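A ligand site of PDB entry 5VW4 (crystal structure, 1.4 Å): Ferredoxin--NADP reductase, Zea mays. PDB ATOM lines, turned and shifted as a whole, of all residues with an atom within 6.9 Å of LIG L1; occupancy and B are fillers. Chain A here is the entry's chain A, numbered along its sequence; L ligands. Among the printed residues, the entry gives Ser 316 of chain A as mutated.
N of Ser 94 sits at hydrogen-bond distance from O8 of LG2 L2, at 3.0 Å. O of Cys 112 is in hydrogen-bond range of N7 of LG2 L2 (2.9 Å). An oxygen (O1) of LIG L1 lies within hydrogen-bond range of the side-chain hydroxyl of Thr 175. An oxygen (O9) of LG2 L2 sits at hydrogen-bond distance from the backbone NH (N) of Leu 92, 3.4 Å away. The side-chain hydroxyl (OG) of Ser 94 is in hydrogen-bond range of a nitrogen (N8) of LG2 L2 (3.2 Å). O of Thr 175 lies within hydrogen-bond range of N2 of LIG L1 (3.0 Å). A nitrogen (N1) of LIG L1 sits close to the backbone NH (N) of Ser 316 (3.4 Å). OH of Tyr 93 is in hydrogen-bond range of O11 of LG2 L2 (2.7 Å). An oxygen (O9) of LG2 L2 sits at hydrogen-bond distance from the backbone carbonyl oxygen of Leu 92 (2.6 Å). The backbone NH of Gly 176 is in hydrogen-bond range of an oxygen (O1) of LIG L1, 3.3 Å away. The side-chain hydroxyl (OG) of Ser 94 lies within hydrogen-bond range of a nitrogen (N2) of LIG L1 (3.1 Å). The side-chain hydroxyl (OG) of Ser 316 lies within hydrogen-bond range of a nitrogen (N1) of LIG L1 (2.5 Å).
SG of Cys 274 touches C3 of LIG L1 (3.5 Å). Gly 275 touches LIG L1 (O to C1, 3.5 Å). Glu 314 touches LIG L1. Val 315 touches LIG L1 (C to C5, 3.5 Å). Within 4 Å of LIG L1: Ser 94, Thr 175, Gly 176, Cys 274, Gly 275, Glu 314, Val 315 and Ser 316.
An oxygen (O8) of LG2 L2 is in hydrogen-bond range of a nitrogen (N2) of LIG L1, at 3.1 Å.
The backbone carbonyl oxygen (O) of Gly 275 sits at hydrogen-bond distance from the backbone NH (N) of Ser 316 (3.4 Å). The backbone carbonyl oxygen (O) of Phe 273 lies within hydrogen-bond range of the backbone NH (N) of Glu 314 (2.9 Å). N of Thr 173 sits at hydrogen-bond distance from O of Cys 274, at 3.3 Å. O of Ser 316 sits at hydrogen-bond distance from N of Lys 277, 2.7 Å away. The backbone carbonyl oxygen of Glu 314 lies close to the side-chain sulfur of Cys 274, 3.5 Å away. The side-chain sulfur of Cys 274 sits close to the backbone carbonyl oxygen of Gly 176 (3.5 Å).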
ATOM      1  N   SER A  71     -31.423  14.286  23.826  1.00  0.00           N
ATOM      2  CA  SER A  71     -30.899  15.628  24.014  1.00  0.00           C
ATOM      3  C   SER A  71     -31.839  16.450  24.878  1.00  0.00           C
ATOM      4  O   SER A  71     -33.053  16.236  24.900  1.00  0.00           O
ATOM      5  CB  SER A  71     -30.760  16.350  22.667  1.00  0.00           C
ATOM      6  OG  SER A  71     -29.810  15.695  21.843  1.00  0.00           O
ATOM      7  N   LEU A  92     -29.600  22.487  21.401  1.00  0.00           N
ATOM      8  CA  LEU A  92     -29.685  21.108  21.871  1.00  0.00           C
ATOM      9  C   LEU A  92     -28.336  20.630  22.356  1.00  0.00           C
ATOM     10  O   LEU A  92     -27.296  20.942  21.769  1.00  0.00           O
ATOM     11  CB  LEU A  92     -30.181  20.212  20.737  1.00  0.00           C
ATOM     12  CG  LEU A  92     -31.610  20.481  20.278  1.00  0.00           C
ATOM     13  CD1 LEU A  92     -31.922  19.657  19.041  1.00  0.00           C
ATOM     14  CD2 LEU A  92     -32.604  20.160  21.359  1.00  0.00           C
ATOM     15  N   TYR A  93     -28.357  19.820  23.400  1.00  0.00           N
ATOM     16  CA  TYR A  93     -27.144  19.242  23.973  1.00  0.00           C
ATOM     17  C   TYR A  93     -27.416  17.775  24.254  1.00  0.00           C
ATOM     18  O   TYR A  93     -28.434  17.433  24.847  1.00  0.00           O
ATOM     19  CB  TYR A  93     -26.708  19.973  25.247  1.00  0.00           C
ATOM     20  CG  TYR A  93     -26.281  21.366  24.890  1.00  0.00           C
ATOM     21  CD1 TYR A  93     -25.023  21.589  24.355  1.00  0.00           C
ATOM     22  CD2 TYR A  93     -27.164  22.427  24.920  1.00  0.00           C
ATOM     23  CE1 TYR A  93     -24.621  22.833  23.909  1.00  0.00           C
ATOM     24  CE2 TYR A  93     -26.768  23.692  24.485  1.00  0.00           C
ATOM     25  CZ  TYR A  93     -25.493  23.882  23.970  1.00  0.00           C
ATOM     26  OH  TYR A  93     -25.086  25.119  23.495  1.00  0.00           O
ATOM     27  N   SER A  94     -26.493  16.933  23.818  1.00  0.00           N
ATOM     28  CA  SER A  94     -26.637  15.513  24.019  1.00  0.00           C
ATOM     29  C   SER A  94     -26.448  15.184  25.487  1.00  0.00           C
ATOM     30  O   SER A  94     -25.468  15.569  26.109  1.00  0.00           O
ATOM     31  CB  SER A  94     -25.573  14.762  23.223  1.00  0.00           C
ATOM     32  OG  SER A  94     -25.689  15.020  21.858  1.00  0.00           O
ATOM     33  N   ILE A  95     -27.397  14.454  26.056  1.00  0.00           N
ATOM     34  CA  ILE A  95     -27.293  14.155  27.468  1.00  0.00           C
ATOM     35  C   ILE A  95     -26.162  13.159  27.655  1.00  0.00           C
ATOM     36  O   ILE A  95     -26.094  12.158  26.958  1.00  0.00           O
ATOM     37  CB  ILE A  95     -28.648  13.671  27.989  1.00  0.00           C
ATOM     38  CG1 ILE A  95     -29.677  14.811  27.874  1.00  0.00           C
ATOM     39  CG2 ILE A  95     -28.517  13.251  29.404  1.00  0.00           C
ATOM     40  CD1 ILE A  95     -31.115  14.375  28.026  1.00  0.00           C
ATOM     41  N   CYS A 112     -22.176  17.777  28.173  1.00  0.00           N
ATOM     42  CA  CYS A 112     -20.766  17.869  27.826  1.00  0.00           C
ATOM     43  C   CYS A 112     -20.680  18.939  26.749  1.00  0.00           C
ATOM     44  O   CYS A 112     -21.054  18.684  25.603  1.00  0.00           O
ATOM     45  CB  CYS A 112     -20.339  16.531  27.264  1.00  0.00           C
ATOM     46  SG  CYS A 112     -18.656  16.453  26.717  1.00  0.00           S
ATOM     47  N   MET A 157     -30.381   8.252  18.658  1.00  0.00           N
ATOM     48  CA  MET A 157     -29.320   7.657  19.454  1.00  0.00           C
ATOM     49  C   MET A 157     -29.846   6.871  20.634  1.00  0.00           C
ATOM     50  O   MET A 157     -29.089   6.566  21.558  1.00  0.00           O
ATOM     51  CB  MET A 157     -28.342   8.726  19.917  1.00  0.00           C
ATOM     52  CG  MET A 157     -27.674   9.459  18.751  1.00  0.00           C
ATOM     53  SD  MET A 157     -26.689   8.406  17.665  1.00  0.00           S
ATOM     54  CE  MET A 157     -25.351   8.081  18.779  1.00  0.00           C
ATOM     55  N   THR A 173     -16.259  12.081  18.106  1.00  0.00           N
ATOM     56  CA  THR A 173     -15.269  13.144  18.178  1.00  0.00           C
ATOM     57  C   THR A 173     -15.768  14.180  19.170  1.00  0.00           C
ATOM     58  O   THR A 173     -16.951  14.542  19.168  1.00  0.00           O
ATOM     59  CB  THR A 173     -14.982  13.788  16.826  1.00  0.00           C
ATOM     60  OG1 THR A 173     -16.189  14.308  16.242  1.00  0.00           O
ATOM     61  CG2 THR A 173     -14.328  12.776  15.885  1.00  0.00           C
ATOM     62  N   GLY A 174     -14.849  14.633  20.017  1.00  0.00           N
ATOM     63  CA  GLY A 174     -15.158  15.693  20.958  1.00  0.00           C
ATOM     64  C   GLY A 174     -16.378  15.382  21.778  1.00  0.00           C
ATOM     65  O   GLY A 174     -16.525  14.288  22.334  1.00  0.00           O
ATOM     66  N   THR A 175     -17.277  16.351  21.850  1.00  0.00           N
ATOM     67  CA  THR A 175     -18.449  16.219  22.696  1.00  0.00           C
ATOM     68  C   THR A 175     -19.381  15.134  22.198  1.00  0.00           C
ATOM     69  O   THR A 175     -20.380  14.835  22.860  1.00  0.00           O
ATOM     70  CB  THR A 175     -19.221  17.542  22.775  1.00  0.00           C
ATOM     71  OG1 THR A 175     -19.508  18.013  21.462  1.00  0.00           O
ATOM     72  CG2 THR A 175     -18.394  18.595  23.507  1.00  0.00           C
ATOM     73  N   GLY A 176     -19.116  14.591  21.009  1.00  0.00           N
ATOM     74  CA  GLY A 176     -19.861  13.445  20.544  1.00  0.00           C
ATOM     75  C   GLY A 176     -19.766  12.258  21.467  1.00  0.00           C
ATOM     76  O   GLY A 176     -20.554  11.318  21.332  1.00  0.00           O
ATOM     77  N   VAL A 177     -18.810  12.266  22.403  1.00  0.00           N
ATOM     78  CA  VAL A 177     -18.723  11.200  23.382  1.00  0.00           C
ATOM     79  C   VAL A 177     -19.936  11.167  24.307  1.00  0.00           C
ATOM     80  O   VAL A 177     -20.188  10.140  24.945  1.00  0.00           O
ATOM     81  CB  VAL A 177     -17.412  11.352  24.169  1.00  0.00           C
ATOM     82  CG1 VAL A 177     -17.514  12.435  25.222  1.00  0.00           C
ATOM     83  CG2 VAL A 177     -17.019  10.021  24.761  1.00  0.00           C
ATOM     84  N   ALA A 178     -20.704  12.255  24.385  1.00  0.00           N
ATOM     85  CA  ALA A 178     -21.755  12.394  25.390  1.00  0.00           C
ATOM     86  C   ALA A 178     -22.726  11.222  25.465  1.00  0.00           C
ATOM     87  O   ALA A 178     -22.877  10.617  26.556  1.00  0.00           O
ATOM     88  CB  ALA A 178     -22.518  13.711  25.183  1.00  0.00           C
ATOM     89  N   PRO A 179     -23.428  10.850  24.384  1.00  0.00           N
ATOM     90  CA  PRO A 179     -24.362   9.728  24.511  1.00  0.00           C
ATOM     91  C   PRO A 179     -23.655   8.459  24.931  1.00  0.00           C
ATOM     92  O   PRO A 179     -24.244   7.631  25.622  1.00  0.00           O
ATOM     93  CB  PRO A 179     -24.950   9.569  23.113  1.00  0.00           C
ATOM     94  CG  PRO A 179     -23.954  10.181  22.221  1.00  0.00           C
ATOM     95  CD  PRO A 179     -23.401  11.358  23.007  1.00  0.00           C
ATOM     96  N   PHE A 273     -22.277   7.142  15.369  1.00  0.00           N
ATOM     97  CA  PHE A 273     -21.386   8.263  15.101  1.00  0.00           C
ATOM     98  C   PHE A 273     -22.007   9.494  15.717  1.00  0.00           C
ATOM     99  O   PHE A 273     -23.178   9.789  15.476  1.00  0.00           O
ATOM    100  CB  PHE A 273     -21.213   8.498  13.612  1.00  0.00           C
ATOM    101  CG  PHE A 273     -20.645   7.322  12.880  1.00  0.00           C
ATOM    102  CD1 PHE A 273     -21.467   6.313  12.424  1.00  0.00           C
ATOM    103  CD2 PHE A 273     -19.284   7.205  12.712  1.00  0.00           C
ATOM    104  CE1 PHE A 273     -20.932   5.242  11.744  1.00  0.00           C
ATOM    105  CE2 PHE A 273     -18.753   6.126  12.036  1.00  0.00           C
ATOM    106  CZ  PHE A 273     -19.569   5.138  11.580  1.00  0.00           C
ATOM    107  N   CYS A 274     -21.215  10.218  16.490  1.00  0.00           N
ATOM    108  CA  CYS A 274     -21.735  11.401  17.163  1.00  0.00           C
ATOM    109  C   CYS A 274     -20.628  12.425  17.276  1.00  0.00           C
ATOM    110  O   CYS A 274     -19.479  12.092  17.562  1.00  0.00           O
ATOM    111  CB  CYS A 274     -22.308  11.024  18.530  1.00  0.00           C
ATOM    112  SG  CYS A 274     -23.228  12.323  19.277  1.00  0.00           S
ATOM    113  N   GLY A 275     -20.992  13.673  17.058  1.00  0.00           N
ATOM    114  CA  GLY A 275     -20.098  14.796  17.161  1.00  0.00           C
ATOM    115  C   GLY A 275     -20.438  15.815  16.104  1.00  0.00           C
ATOM    116  O   GLY A 275     -21.539  15.841  15.571  1.00  0.00           O
ATOM    117  N   LEU A 276     -19.471  16.659  15.793  1.00  0.00           N
ATOM    118  CA  LEU A 276     -19.706  17.633  14.733  1.00  0.00           C
ATOM    119  C   LEU A 276     -19.602  16.966  13.377  1.00  0.00           C
ATOM    120  O   LEU A 276     -18.821  16.030  13.164  1.00  0.00           O
ATOM    121  CB  LEU A 276     -18.741  18.809  14.877  1.00  0.00           C
ATOM    122  CG  LEU A 276     -18.884  19.497  16.242  1.00  0.00           C
ATOM    123  CD1 LEU A 276     -17.925  20.647  16.378  1.00  0.00           C
ATOM    124  CD2 LEU A 276     -20.322  19.996  16.461  1.00  0.00           C
ATOM    125  N   LYS A 277     -20.400  17.475  12.436  1.00  0.00           N
ATOM    126  CA  LYS A 277     -20.595  16.768  11.170  1.00  0.00           C
ATOM    127  C   LYS A 277     -19.334  16.704  10.328  1.00  0.00           C
ATOM    128  O   LYS A 277     -19.237  15.820   9.471  1.00  0.00           O
ATOM    129  CB  LYS A 277     -21.749  17.382  10.382  1.00  0.00           C
ATOM    130  CG  LYS A 277     -21.472  18.776   9.889  1.00  0.00           C
ATOM    131  CD  LYS A 277     -22.710  19.408   9.261  1.00  0.00           C
ATOM    132  CE  LYS A 277     -22.517  20.906   9.039  1.00  0.00           C
ATOM    133  NZ  LYS A 277     -23.760  21.560   8.513  1.00  0.00           N
ATOM    134  N   GLU A 314     -25.743  10.893  14.587  1.00  0.00           N
ATOM    135  CA  GLU A 314     -26.292  12.167  15.031  1.00  0.00           C
ATOM    136  C   GLU A 314     -25.135  13.151  15.111  1.00  0.00           C
ATOM    137  O   GLU A 314     -24.309  13.105  16.026  1.00  0.00           O
ATOM    138  CB  GLU A 314     -27.076  12.064  16.331  1.00  0.00           C
ATOM    139  CG  GLU A 314     -28.054  13.265  16.448  1.00  0.00           C
ATOM    140  CD  GLU A 314     -29.005  13.171  17.596  1.00  0.00           C
ATOM    141  OE1 GLU A 314     -28.630  12.599  18.624  1.00  0.00           O
ATOM    142  OE2 GLU A 314     -30.123  13.691  17.468  1.00  0.00           O
ATOM    143  N   VAL A 315     -25.046  14.002  14.104  1.00  0.00           N
ATOM    144  CA  VAL A 315     -23.983  14.986  13.983  1.00  0.00           C
ATOM    145  C   VAL A 315     -24.626  16.287  13.558  1.00  0.00           C
ATOM    146  O   VAL A 315     -25.759  16.324  13.088  1.00  0.00           O
ATOM    147  CB  VAL A 315     -22.916  14.537  12.963  1.00  0.00           C
ATOM    148  CG1 VAL A 315     -22.232  13.249  13.463  1.00  0.00           C
ATOM    149  CG2 VAL A 315     -23.507  14.337  11.578  1.00  0.00           C
ATOM    150  N   SER A 316     -23.886  17.379  13.730  1.00  0.00           N
ATOM    151  CA  SER A 316     -24.402  18.680  13.358  1.00  0.00           C
ATOM    152  C   SER A 316     -23.281  19.640  13.045  1.00  0.00           C
ATOM    153  O   SER A 316     -22.106  19.392  13.328  1.00  0.00           O
ATOM    154  CB  SER A 316     -25.273  19.244  14.470  1.00  0.00           C
ATOM    155  OG  SER A 316     -24.466  19.603  15.587  1.00  0.00           O
ATOM    156  OXT SER A 316     -23.550  20.714  12.505  1.00  0.00           O
HETATM  157  N1  LIG L   1     -24.263  17.586  17.097  1.00  0.00           N
HETATM  158  C1  LIG L   1     -23.365  17.435  18.076  1.00  0.00           C
HETATM  159  C2  LIG L   1     -23.481  16.397  18.994  1.00  0.00           C
HETATM  160  C3  LIG L   1     -24.526  15.509  18.886  1.00  0.00           C
HETATM  161  C4  LIG L   1     -25.441  15.678  17.860  1.00  0.00           C
HETATM  162  C5  LIG L   1     -25.296  16.735  16.978  1.00  0.00           C
HETATM  163  C6  LIG L   1     -22.461  16.263  20.074  1.00  0.00           C
HETATM  164  O1  LIG L   1     -21.379  16.786  19.912  1.00  0.00           O
HETATM  165  N2  LIG L   1     -22.744  15.592  21.186  1.00  0.00           N
HETATM  166  P1  LG2 L   2     -24.463  30.274  18.705  1.00  0.00           P
HETATM  167  O1  LG2 L   2     -24.706  31.518  19.459  1.00  0.00           O
HETATM  168  O2  LG2 L   2     -25.632  29.528  18.147  1.00  0.00           O
HETATM  169  O3  LG2 L   2     -23.424  30.616  17.544  1.00  0.00           O
HETATM  170  C1  LG2 L   2     -23.126  29.610  16.582  1.00  0.00           C
HETATM  171  C2  LG2 L   2     -21.703  29.806  16.082  1.00  0.00           C
HETATM  172  O4  LG2 L   2     -21.613  31.069  15.390  1.00  0.00           O
HETATM  173  C3  LG2 L   2     -20.657  29.848  17.188  1.00  0.00           C
HETATM  174  O5  LG2 L   2     -19.506  29.105  16.774  1.00  0.00           O
HETATM  175  C4  LG2 L   2     -20.276  31.325  17.289  1.00  0.00           C
HETATM  176  O6  LG2 L   2     -18.945  31.537  17.786  1.00  0.00           O
HETATM  177  C5  LG2 L   2     -20.449  31.757  15.843  1.00  0.00           C
HETATM  178  N1  LG2 L   2     -20.733  33.182  15.606  1.00  0.00           N
HETATM  179  C6  LG2 L   2     -21.661  33.933  16.224  1.00  0.00           C
HETATM  180  N2  LG2 L   2     -21.645  35.196  15.714  1.00  0.00           N
HETATM  181  C7  LG2 L   2     -20.712  35.235  14.760  1.00  0.00           C
HETATM  182  C8  LG2 L   2     -20.175  36.245  13.832  1.00  0.00           C
HETATM  183  N3  LG2 L   2     -20.687  37.490  13.841  1.00  0.00           N
HETATM  184  N4  LG2 L   2     -19.184  35.867  13.010  1.00  0.00           N
HETATM  185  C9  LG2 L   2     -18.668  34.630  12.996  1.00  0.00           C
HETATM  186  N5  LG2 L   2     -19.117  33.655  13.815  1.00  0.00           N
HETATM  187  C10 LG2 L   2     -20.106  33.908  14.699  1.00  0.00           C
HETATM  188  N6  LG2 L   2     -22.758  20.898  21.352  1.00  0.00           N
HETATM  189  C11 LG2 L   2     -22.028  20.535  22.413  1.00  0.00           C
HETATM  190  O7  LG2 L   2     -21.080  21.255  22.778  1.00  0.00           O
HETATM  191  N7  LG2 L   2     -22.296  19.421  23.102  1.00  0.00           N
HETATM  192  C12 LG2 L   2     -23.303  18.590  22.799  1.00  0.00           C
HETATM  193  O8  LG2 L   2     -23.552  17.586  23.459  1.00  0.00           O
HETATM  194  C13 LG2 L   2     -24.139  18.927  21.655  1.00  0.00           C
HETATM  195  N8  LG2 L   2     -25.176  18.155  21.281  1.00  0.00           N
HETATM  196  C14 LG2 L   2     -25.951  18.523  20.238  1.00  0.00           C
HETATM  197  C15 LG2 L   2     -27.021  17.728  19.841  1.00  0.00           C
HETATM  198  C16 LG2 L   2     -27.797  18.058  18.751  1.00  0.00           C
HETATM  199  C17 LG2 L   2     -28.938  17.167  18.349  1.00  0.00           C
HETATM  200  C18 LG2 L   2     -27.476  19.252  17.983  1.00  0.00           C
HETATM  201  C19 LG2 L   2     -28.296  19.629  16.770  1.00  0.00           C
HETATM  202  C20 LG2 L   2     -26.420  20.051  18.353  1.00  0.00           C
HETATM  203  C21 LG2 L   2     -25.645  19.731  19.461  1.00  0.00           C
HETATM  204  N9  LG2 L   2     -24.576  20.547  19.892  1.00  0.00           N
HETATM  205  C22 LG2 L   2     -23.793  20.153  20.962  1.00  0.00           C
HETATM  206  C23 LG2 L   2     -24.357  21.886  19.347  1.00  0.00           C
HETATM  207  C24 LG2 L   2     -25.132  22.914  20.180  1.00  0.00           C
HETATM  208  O9  LG2 L   2     -26.522  22.716  20.009  1.00  0.00           O
HETATM  209  C25 LG2 L   2     -24.893  24.368  19.743  1.00  0.00           C
HETATM  210  O10 LG2 L   2     -25.154  24.511  18.346  1.00  0.00           O
HETATM  211  C26 LG2 L   2     -23.483  24.807  20.051  1.00  0.00           C
HETATM  212  O11 LG2 L   2     -23.295  24.678  21.460  1.00  0.00           O
HETATM  213  C27 LG2 L   2     -23.256  26.267  19.680  1.00  0.00           C
HETATM  214  O12 LG2 L   2     -24.326  27.026  20.227  1.00  0.00           O
HETATM  215  P2  LG2 L   2     -24.060  28.457  20.873  1.00  0.00           P
HETATM  216  O13 LG2 L   2     -25.373  28.971  21.366  1.00  0.00           O
HETATM  217  O14 LG2 L   2     -22.895  28.404  21.796  1.00  0.00           O
HETATM  218  O15 LG2 L   2     -23.524  29.302  19.589  1.00  0.00           O
